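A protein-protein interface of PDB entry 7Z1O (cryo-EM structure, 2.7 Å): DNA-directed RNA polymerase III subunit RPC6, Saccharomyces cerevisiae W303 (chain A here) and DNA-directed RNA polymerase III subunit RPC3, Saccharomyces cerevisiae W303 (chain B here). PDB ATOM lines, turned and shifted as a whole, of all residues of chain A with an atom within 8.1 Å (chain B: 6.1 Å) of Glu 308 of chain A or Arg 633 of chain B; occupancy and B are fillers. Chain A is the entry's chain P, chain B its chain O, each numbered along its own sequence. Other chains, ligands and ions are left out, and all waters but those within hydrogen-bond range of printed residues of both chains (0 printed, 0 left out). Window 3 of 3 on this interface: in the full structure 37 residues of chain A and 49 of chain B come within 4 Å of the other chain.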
ATOM      1  N   ALA A 302      23.261 -25.480  19.737  1.00  0.00           N
ATOM      2  CA  ALA A 302      22.875 -24.078  19.789  1.00  0.00           C
ATOM      3  C   ALA A 302      21.873 -23.750  18.690  1.00  0.00           C
ATOM      4  O   ALA A 302      21.870 -24.355  17.615  1.00  0.00           O
ATOM      5  CB  ALA A 302      24.102 -23.178  19.656  1.00  0.00           C
ATOM      6  N   SER A 303      21.010 -22.779  18.976  1.00  0.00           N
ATOM      7  CA  SER A 303      20.041 -22.322  17.994  1.00  0.00           C
ATOM      8  C   SER A 303      20.741 -21.581  16.862  1.00  0.00           C
ATOM      9  O   SER A 303      21.852 -21.066  17.016  1.00  0.00           O
ATOM     10  CB  SER A 303      19.002 -21.415  18.651  1.00  0.00           C
ATOM     11  OG  SER A 303      18.235 -20.729  17.677  1.00  0.00           O
ATOM     12  N   HIS A 305      21.367 -18.626  13.938  1.00  0.00           N
ATOM     13  CA  HIS A 305      21.573 -17.177  14.044  1.00  0.00           C
ATOM     14  C   HIS A 305      22.169 -16.797  15.398  1.00  0.00           C
ATOM     15  O   HIS A 305      21.822 -15.772  15.986  1.00  0.00           O
ATOM     16  CB  HIS A 305      20.280 -16.401  13.774  1.00  0.00           C
ATOM     17  CG  HIS A 305      19.607 -16.775  12.491  1.00  0.00           C
ATOM     18  ND1 HIS A 305      18.808 -17.891  12.368  1.00  0.00           N
ATOM     19  CD2 HIS A 305      19.621 -16.185  11.272  1.00  0.00           C
ATOM     20  CE1 HIS A 305      18.355 -17.971  11.129  1.00  0.00           C
ATOM     21  NE2 HIS A 305      18.833 -16.947  10.444  1.00  0.00           N
ATOM     22  N   ASP A 306      23.074 -17.635  15.896  1.00  0.00           N
ATOM     23  CA  ASP A 306      23.833 -17.361  17.110  1.00  0.00           C
ATOM     24  C   ASP A 306      25.280 -17.103  16.715  1.00  0.00           C
ATOM     25  O   ASP A 306      25.973 -18.017  16.254  1.00  0.00           O
ATOM     26  CB  ASP A 306      23.736 -18.524  18.096  1.00  0.00           C
ATOM     27  CG  ASP A 306      23.993 -18.098  19.527  1.00  0.00           C
ATOM     28  OD1 ASP A 306      24.081 -16.879  19.779  1.00  0.00           O
ATOM     29  OD2 ASP A 306      24.100 -18.981  20.402  1.00  0.00           O
ATOM     30  N   LYS A 307      25.730 -15.861  16.894  1.00  0.00           N
ATOM     31  CA  LYS A 307      27.064 -15.483  16.441  1.00  0.00           C
ATOM     32  C   LYS A 307      28.147 -16.051  17.351  1.00  0.00           C
ATOM     33  O   LYS A 307      29.204 -16.480  16.875  1.00  0.00           O
ATOM     34  CB  LYS A 307      27.179 -13.961  16.362  1.00  0.00           C
ATOM     35  CG  LYS A 307      26.560 -13.346  15.118  1.00  0.00           C
ATOM     36  CD  LYS A 307      25.116 -12.941  15.367  1.00  0.00           C
ATOM     37  CE  LYS A 307      24.589 -12.047  14.257  1.00  0.00           C
ATOM     38  NZ  LYS A 307      23.185 -11.622  14.517  1.00  0.00           N
ATOM     39  N   GLU A 308      27.901 -16.063  18.660  1.00  0.00           N
ATOM     40  CA  GLU A 308      28.926 -16.407  19.646  1.00  0.00           C
ATOM     41  C   GLU A 308      28.865 -17.904  19.988  1.00  0.00           C
ATOM     42  O   GLU A 308      28.699 -18.339  21.129  1.00  0.00           O
ATOM     43  CB  GLU A 308      28.795 -15.484  20.858  1.00  0.00           C
ATOM     44  CG  GLU A 308      27.547 -15.655  21.729  1.00  0.00           C
ATOM     45  CD  GLU A 308      26.344 -14.893  21.222  1.00  0.00           C
ATOM     46  OE1 GLU A 308      26.348 -14.458  20.051  1.00  0.00           O
ATOM     47  OE2 GLU A 308      25.379 -14.752  21.997  1.00  0.00           O
ATOM     48  N   VAL A 309      29.084 -18.707  18.954  1.00  0.00           N
ATOM     49  CA  VAL A 309      29.078 -20.161  19.063  1.00  0.00           C
ATOM     50  C   VAL A 309      30.489 -20.669  18.778  1.00  0.00           C
ATOM     51  O   VAL A 309      31.164 -20.175  17.866  1.00  0.00           O
ATOM     52  CB  VAL A 309      28.019 -20.791  18.133  1.00  0.00           C
ATOM     53  CG1 VAL A 309      28.303 -20.496  16.675  1.00  0.00           C
ATOM     54  CG2 VAL A 309      27.937 -22.290  18.352  1.00  0.00           C
ATOM     55  N   VAL A 310      30.952 -21.608  19.599  1.00  0.00           N
ATOM     56  CA  VAL A 310      32.345 -22.043  19.584  1.00  0.00           C
ATOM     57  C   VAL A 310      32.477 -23.287  18.718  1.00  0.00           C
ATOM     58  O   VAL A 310      31.773 -24.281  18.928  1.00  0.00           O
ATOM     59  CB  VAL A 310      32.849 -22.310  21.010  1.00  0.00           C
ATOM     60  CG1 VAL A 310      34.260 -22.870  20.981  1.00  0.00           C
ATOM     61  CG2 VAL A 310      32.795 -21.041  21.837  1.00  0.00           C
ATOM     62  N   TYR A 311      33.389 -23.236  17.751  1.00  0.00           N
ATOM     63  CA  TYR A 311      33.612 -24.324  16.809  1.00  0.00           C
ATOM     64  C   TYR A 311      34.987 -24.935  17.038  1.00  0.00           C
ATOM     65  O   TYR A 311      35.970 -24.212  17.232  1.00  0.00           O
ATOM     66  CB  TYR A 311      33.504 -23.833  15.367  1.00  0.00           C
ATOM     67  CG  TYR A 311      32.093 -23.613  14.882  1.00  0.00           C
ATOM     68  CD1 TYR A 311      31.284 -24.683  14.533  1.00  0.00           C
ATOM     69  CD2 TYR A 311      31.577 -22.333  14.756  1.00  0.00           C
ATOM     70  CE1 TYR A 311      29.995 -24.485  14.085  1.00  0.00           C
ATOM     71  CE2 TYR A 311      30.295 -22.127  14.304  1.00  0.00           C
ATOM     72  CZ  TYR A 311      29.506 -23.204  13.973  1.00  0.00           C
ATOM     73  OH  TYR A 311      28.223 -22.996  13.525  1.00  0.00           O
ATOM     74  N   LEU B 588      35.969 -15.629  21.697  1.00  0.00           N
ATOM     75  CA  LEU B 588      34.717 -15.362  22.397  1.00  0.00           C
ATOM     76  C   LEU B 588      34.774 -14.028  23.137  1.00  0.00           C
ATOM     77  O   LEU B 588      33.834 -13.222  23.070  1.00  0.00           O
ATOM     78  CB  LEU B 588      34.428 -16.511  23.360  1.00  0.00           C
ATOM     79  CG  LEU B 588      32.990 -16.806  23.761  1.00  0.00           C
ATOM     80  CD1 LEU B 588      32.188 -17.231  22.552  1.00  0.00           C
ATOM     81  CD2 LEU B 588      32.989 -17.893  24.808  1.00  0.00           C
ATOM     82  N   LYS B 591      34.614 -11.195  20.588  1.00  0.00           N
ATOM     83  CA  LYS B 591      33.249 -10.970  20.121  1.00  0.00           C
ATOM     84  C   LYS B 591      32.421 -10.228  21.164  1.00  0.00           C
ATOM     85  O   LYS B 591      31.641  -9.328  20.822  1.00  0.00           O
ATOM     86  CB  LYS B 591      32.592 -12.301  19.767  1.00  0.00           C
ATOM     87  CG  LYS B 591      32.979 -12.842  18.406  1.00  0.00           C
ATOM     88  CD  LYS B 591      32.424 -14.237  18.199  1.00  0.00           C
ATOM     89  CE  LYS B 591      32.770 -14.772  16.823  1.00  0.00           C
ATOM     90  NZ  LYS B 591      32.514 -16.233  16.721  1.00  0.00           N
ATOM     91  N   LEU B 595      30.740  -6.535  20.653  1.00  0.00           N
ATOM     92  CA  LEU B 595      29.313  -6.294  20.861  1.00  0.00           C
ATOM     93  C   LEU B 595      29.080  -5.153  21.845  1.00  0.00           C
ATOM     94  O   LEU B 595      28.222  -4.286  21.623  1.00  0.00           O
ATOM     95  CB  LEU B 595      28.642  -7.576  21.351  1.00  0.00           C
ATOM     96  CG  LEU B 595      27.195  -7.465  21.824  1.00  0.00           C
ATOM     97  CD1 LEU B 595      26.284  -7.103  20.665  1.00  0.00           C
ATOM     98  CD2 LEU B 595      26.755  -8.764  22.472  1.00  0.00           C
ATOM     99  N   ASN B 599      27.234  -1.517  21.150  1.00  0.00           N
ATOM    100  CA  ASN B 599      26.042  -1.072  21.866  1.00  0.00           C
ATOM    101  C   ASN B 599      26.372  -0.200  23.078  1.00  0.00           C
ATOM    102  O   ASN B 599      25.547  -0.087  23.994  1.00  0.00           O
ATOM    103  CB  ASN B 599      25.203  -2.276  22.290  1.00  0.00           C
ATOM    104  CG  ASN B 599      24.436  -2.883  21.136  1.00  0.00           C
ATOM    105  OD1 ASN B 599      23.350  -2.423  20.787  1.00  0.00           O
ATOM    106  ND2 ASN B 599      24.997  -3.924  20.537  1.00  0.00           N
ATOM    107  N   LYS B 628      17.793  -6.494  26.174  1.00  0.00           N
ATOM    108  CA  LYS B 628      17.463  -7.899  26.387  1.00  0.00           C
ATOM    109  C   LYS B 628      18.419  -8.807  25.625  1.00  0.00           C
ATOM    110  O   LYS B 628      19.067  -9.691  26.208  1.00  0.00           O
ATOM    111  CB  LYS B 628      16.032  -8.137  25.895  1.00  0.00           C
ATOM    112  CG  LYS B 628      15.465  -9.527  26.062  1.00  0.00           C
ATOM    113  CD  LYS B 628      15.328  -9.897  27.501  1.00  0.00           C
ATOM    114  CE  LYS B 628      14.212  -9.046  28.084  1.00  0.00           C
ATOM    115  NZ  LYS B 628      13.909  -9.342  29.506  1.00  0.00           N
ATOM    116  N   MET B 629      18.544  -8.567  24.316  1.00  0.00           N
ATOM    117  CA  MET B 629      19.395  -9.400  23.473  1.00  0.00           C
ATOM    118  C   MET B 629      20.861  -9.275  23.858  1.00  0.00           C
ATOM    119  O   MET B 629      21.587 -10.276  23.894  1.00  0.00           O
ATOM    120  CB  MET B 629      19.201  -9.035  22.002  1.00  0.00           C
ATOM    121  CG  MET B 629      17.815  -9.329  21.441  1.00  0.00           C
ATOM    122  SD  MET B 629      17.347 -11.075  21.471  1.00  0.00           S
ATOM    123  CE  MET B 629      16.243 -11.152  22.880  1.00  0.00           C
ATOM    124  N   VAL B 630      21.317  -8.054  24.153  1.00  0.00           N
ATOM    125  CA  VAL B 630      22.725  -7.838  24.473  1.00  0.00           C
ATOM    126  C   VAL B 630      23.099  -8.552  25.766  1.00  0.00           C
ATOM    127  O   VAL B 630      24.138  -9.221  25.844  1.00  0.00           O
ATOM    128  CB  VAL B 630      23.031  -6.331  24.542  1.00  0.00           C
ATOM    129  CG1 VAL B 630      24.320  -6.081  25.298  1.00  0.00           C
ATOM    130  CG2 VAL B 630      23.118  -5.748  23.142  1.00  0.00           C
ATOM    131  N   ASN B 631      22.253  -8.441  26.795  1.00  0.00           N
ATOM    132  CA  ASN B 631      22.565  -9.090  28.063  1.00  0.00           C
ATOM    133  C   ASN B 631      22.485 -10.606  27.947  1.00  0.00           C
ATOM    134  O   ASN B 631      23.305 -11.321  28.538  1.00  0.00           O
ATOM    135  CB  ASN B 631      21.638  -8.576  29.159  1.00  0.00           C
ATOM    136  CG  ASN B 631      22.111  -7.262  29.738  1.00  0.00           C
ATOM    137  OD1 ASN B 631      22.744  -7.221  30.790  1.00  0.00           O
ATOM    138  ND2 ASN B 631      21.828  -6.180  29.034  1.00  0.00           N
ATOM    139  N   GLU B 632      21.517 -11.121  27.178  1.00  0.00           N
ATOM    140  CA  GLU B 632      21.456 -12.564  26.964  1.00  0.00           C
ATOM    141  C   GLU B 632      22.698 -13.068  26.236  1.00  0.00           C
ATOM    142  O   GLU B 632      23.258 -14.112  26.594  1.00  0.00           O
ATOM    143  CB  GLU B 632      20.190 -12.928  26.188  1.00  0.00           C
ATOM    144  CG  GLU B 632      20.008 -14.418  25.953  1.00  0.00           C
ATOM    145  CD  GLU B 632      19.736 -15.186  27.232  1.00  0.00           C
ATOM    146  OE1 GLU B 632      19.155 -14.599  28.169  1.00  0.00           O
ATOM    147  OE2 GLU B 632      20.100 -16.378  27.300  1.00  0.00           O
ATOM    148  N   ARG B 633      23.156 -12.323  25.224  1.00  0.00           N
ATOM    149  CA  ARG B 633      24.356 -12.717  24.493  1.00  0.00           C
ATOM    150  C   ARG B 633      25.592 -12.671  25.383  1.00  0.00           C
ATOM    151  O   ARG B 633      26.457 -13.549  25.298  1.00  0.00           O
ATOM    152  CB  ARG B 633      24.537 -11.825  23.266  1.00  0.00           C
ATOM    153  CG  ARG B 633      23.571 -12.139  22.136  1.00  0.00           C
ATOM    154  CD  ARG B 633      23.656 -11.114  21.026  1.00  0.00           C
ATOM    155  NE  ARG B 633      24.900 -11.224  20.276  1.00  0.00           N
ATOM    156  CZ  ARG B 633      25.254 -10.406  19.296  1.00  0.00           C
ATOM    157  NH1 ARG B 633      24.476  -9.406  18.916  1.00  0.00           N
ATOM    158  NH2 ARG B 633      26.416 -10.598  18.678  1.00  0.00           N
ATOM    159  N   GLU B 634      25.693 -11.656  26.247  1.00  0.00           N
ATOM    160  CA  GLU B 634      26.837 -11.563  27.153  1.00  0.00           C
ATOM    161  C   GLU B 634      26.848 -12.709  28.162  1.00  0.00           C
ATOM    162  O   GLU B 634      27.907 -13.288  28.448  1.00  0.00           O
ATOM    163  CB  GLU B 634      26.825 -10.213  27.868  1.00  0.00           C
ATOM    164  CG  GLU B 634      28.049  -9.951  28.722  1.00  0.00           C
ATOM    165  CD  GLU B 634      28.147  -8.507  29.171  1.00  0.00           C
ATOM    166  OE1 GLU B 634      27.376  -7.670  28.657  1.00  0.00           O
ATOM    167  OE2 GLU B 634      28.994  -8.208  30.038  1.00  0.00           O
ATOM    168  N   LEU B 635      25.677 -13.051  28.709  1.00  0.00           N
ATOM    169  CA  LEU B 635      25.590 -14.187  29.625  1.00  0.00           C
ATOM    170  C   LEU B 635      25.952 -15.492  28.929  1.00  0.00           C
ATOM    171  O   LEU B 635      26.633 -16.345  29.512  1.00  0.00           O
ATOM    172  CB  LEU B 635      24.189 -14.275  30.229  1.00  0.00           C
ATOM    173  CG  LEU B 635      23.980 -13.642  31.606  1.00  0.00           C
ATOM    174  CD1 LEU B 635      24.175 -12.146  31.562  1.00  0.00           C
ATOM    175  CD2 LEU B 635      22.593 -13.974  32.120  1.00  0.00           C
ATOM    176  N   ASN B 636      25.509 -15.668  27.681  1.00  0.00           N
ATOM    177  CA  ASN B 636      25.877 -16.866  26.932  1.00  0.00           C
ATOM    178  C   ASN B 636      27.377 -16.914  26.664  1.00  0.00           C
ATOM    179  O   ASN B 636      27.991 -17.988  26.729  1.00  0.00           O
ATOM    180  CB  ASN B 636      25.092 -16.927  25.622  1.00  0.00           C
ATOM    181  CG  ASN B 636      23.762 -17.634  25.776  1.00  0.00           C
ATOM    182  OD1 ASN B 636      23.671 -18.850  25.618  1.00  0.00           O
ATOM    183  ND2 ASN B 636      22.720 -16.872  26.084  1.00  0.00           N
ATOM    184  N   VAL B 637      27.982 -15.759  26.366  1.00  0.00           N
ATOM    185  CA  VAL B 637      29.428 -15.690  26.155  1.00  0.00           C
ATOM    186  C   VAL B 637      30.168 -16.133  27.409  1.00  0.00           C
ATOM    187  O   VAL B 637      31.100 -16.943  27.347  1.00  0.00           O
ATOM    188  CB  VAL B 637      29.842 -14.267  25.735  1.00  0.00           C
ATOM    189  CG1 VAL B 637      31.326 -14.049  25.962  1.00  0.00           C
ATOM    190  CG2 VAL B 637      29.511 -14.025  24.281  1.00  0.00           C
ATOM    191  N   PHE B 638      29.746 -15.630  28.570  1.00  0.00           N
ATOM    192  CA  PHE B 638      30.453 -15.975  29.801  1.00  0.00           C
ATOM    193  C   PHE B 638      30.215 -17.429  30.200  1.00  0.00           C
ATOM    194  O   PHE B 638      31.114 -18.083  30.743  1.00  0.00           O
ATOM    195  CB  PHE B 638      30.054 -15.020  30.921  1.00  0.00           C
ATOM    196  CG  PHE B 638      30.754 -13.692  30.852  1.00  0.00           C
ATOM    197  CD1 PHE B 638      32.132 -13.626  30.755  1.00  0.00           C
ATOM    198  CD2 PHE B 638      30.034 -12.512  30.881  1.00  0.00           C
ATOM    199  CE1 PHE B 638      32.780 -12.413  30.691  1.00  0.00           C
ATOM    200  CE2 PHE B 638      30.678 -11.294  30.816  1.00  0.00           C
ATOM    201  CZ  PHE B 638      32.052 -11.245  30.723  1.00  0.00           C
ATOM    202  N   ARG B 640      29.738 -19.952  28.036  1.00  0.00           N
ATOM    203  CA  ARG B 640      30.605 -20.728  27.154  1.00  0.00           C
ATOM    204  C   ARG B 640      32.068 -20.582  27.553  1.00  0.00           C
ATOM    205  O   ARG B 640      32.851 -21.529  27.419  1.00  0.00           O
ATOM    206  CB  ARG B 640      30.393 -20.306  25.701  1.00  0.00           C
ATOM    207  CG  ARG B 640      29.207 -20.970  25.036  1.00  0.00           C
ATOM    208  CD  ARG B 640      28.485 -20.030  24.093  1.00  0.00           C
ATOM    209  NE  ARG B 640      27.224 -20.601  23.642  1.00  0.00           N
ATOM    210  CZ  ARG B 640      26.327 -19.956  22.909  1.00  0.00           C
ATOM    211  NH1 ARG B 640      26.521 -18.708  22.520  1.00  0.00           N
ATOM    212  NH2 ARG B 640      25.208 -20.581  22.556  1.00  0.00           N
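NZ of Lys 591 of chain B sits at hydrogen-bond distance from O of Lys 307 of chain A, at 3.3 Å. The side-chain carboxylate of Glu 308 of chain A is in salt-bridge range of the guanidinium group of Arg 633 of chain B, 3.6 Å away. The side-chain carboxylate of Asp 306 of chain A lies within salt-bridge range of the guanidinium group of Arg 640 of chain B. NH1 of Arg 640 of chain B is in hydrogen-bond range of O of Glu 308 of chain A (2.6 Å).
O of Glu 308 of chain A touches CD1 of Leu 588 of chain B, at 3.9 Å. Glu 308 of chain A touches Val 637 of chain B (CG to CG2, 3.6 Å). CG2 of Val 310 of chain A touches CD1 of Leu 588 of chain B (3.9 Å).
Arg 633 of chain B touches just one residue of chain A: Glu 308 (3.2 Å). Printed residues of chain A within 4 Å of Arg 640 of chain B: Asp 306 and Glu 308. Printed residues of chain A within 4 Å of Val 637 of chain B: Glu 308 (3.6 Å). Printed residues of chain A within 4 Å of Lys 591 of chain B: Lys 307 (3.3 Å). Of the printed residues of chain A, Leu 588 of chain B touches Glu 308 and Val 310. Leu 595 of chain B touches none of the printed residues of chain A. Ser 303 of chain A touches none of the printed residues of chain B. The nearest printed residue of chain A that does not touch Lys 591 of chain B is Val 309 of chain A (4.3 Å).
Of the 9 printed residues of chain A, 4 touch a printed residue of chain B. Hydrophobic or aromatic side chains of chain A that line the printed part of chain B: Val 310. Of the 16 printed residues of chain B, 5 touch a printed residue of chain A. Among the printed residues, 7 pairs touch across the chains.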
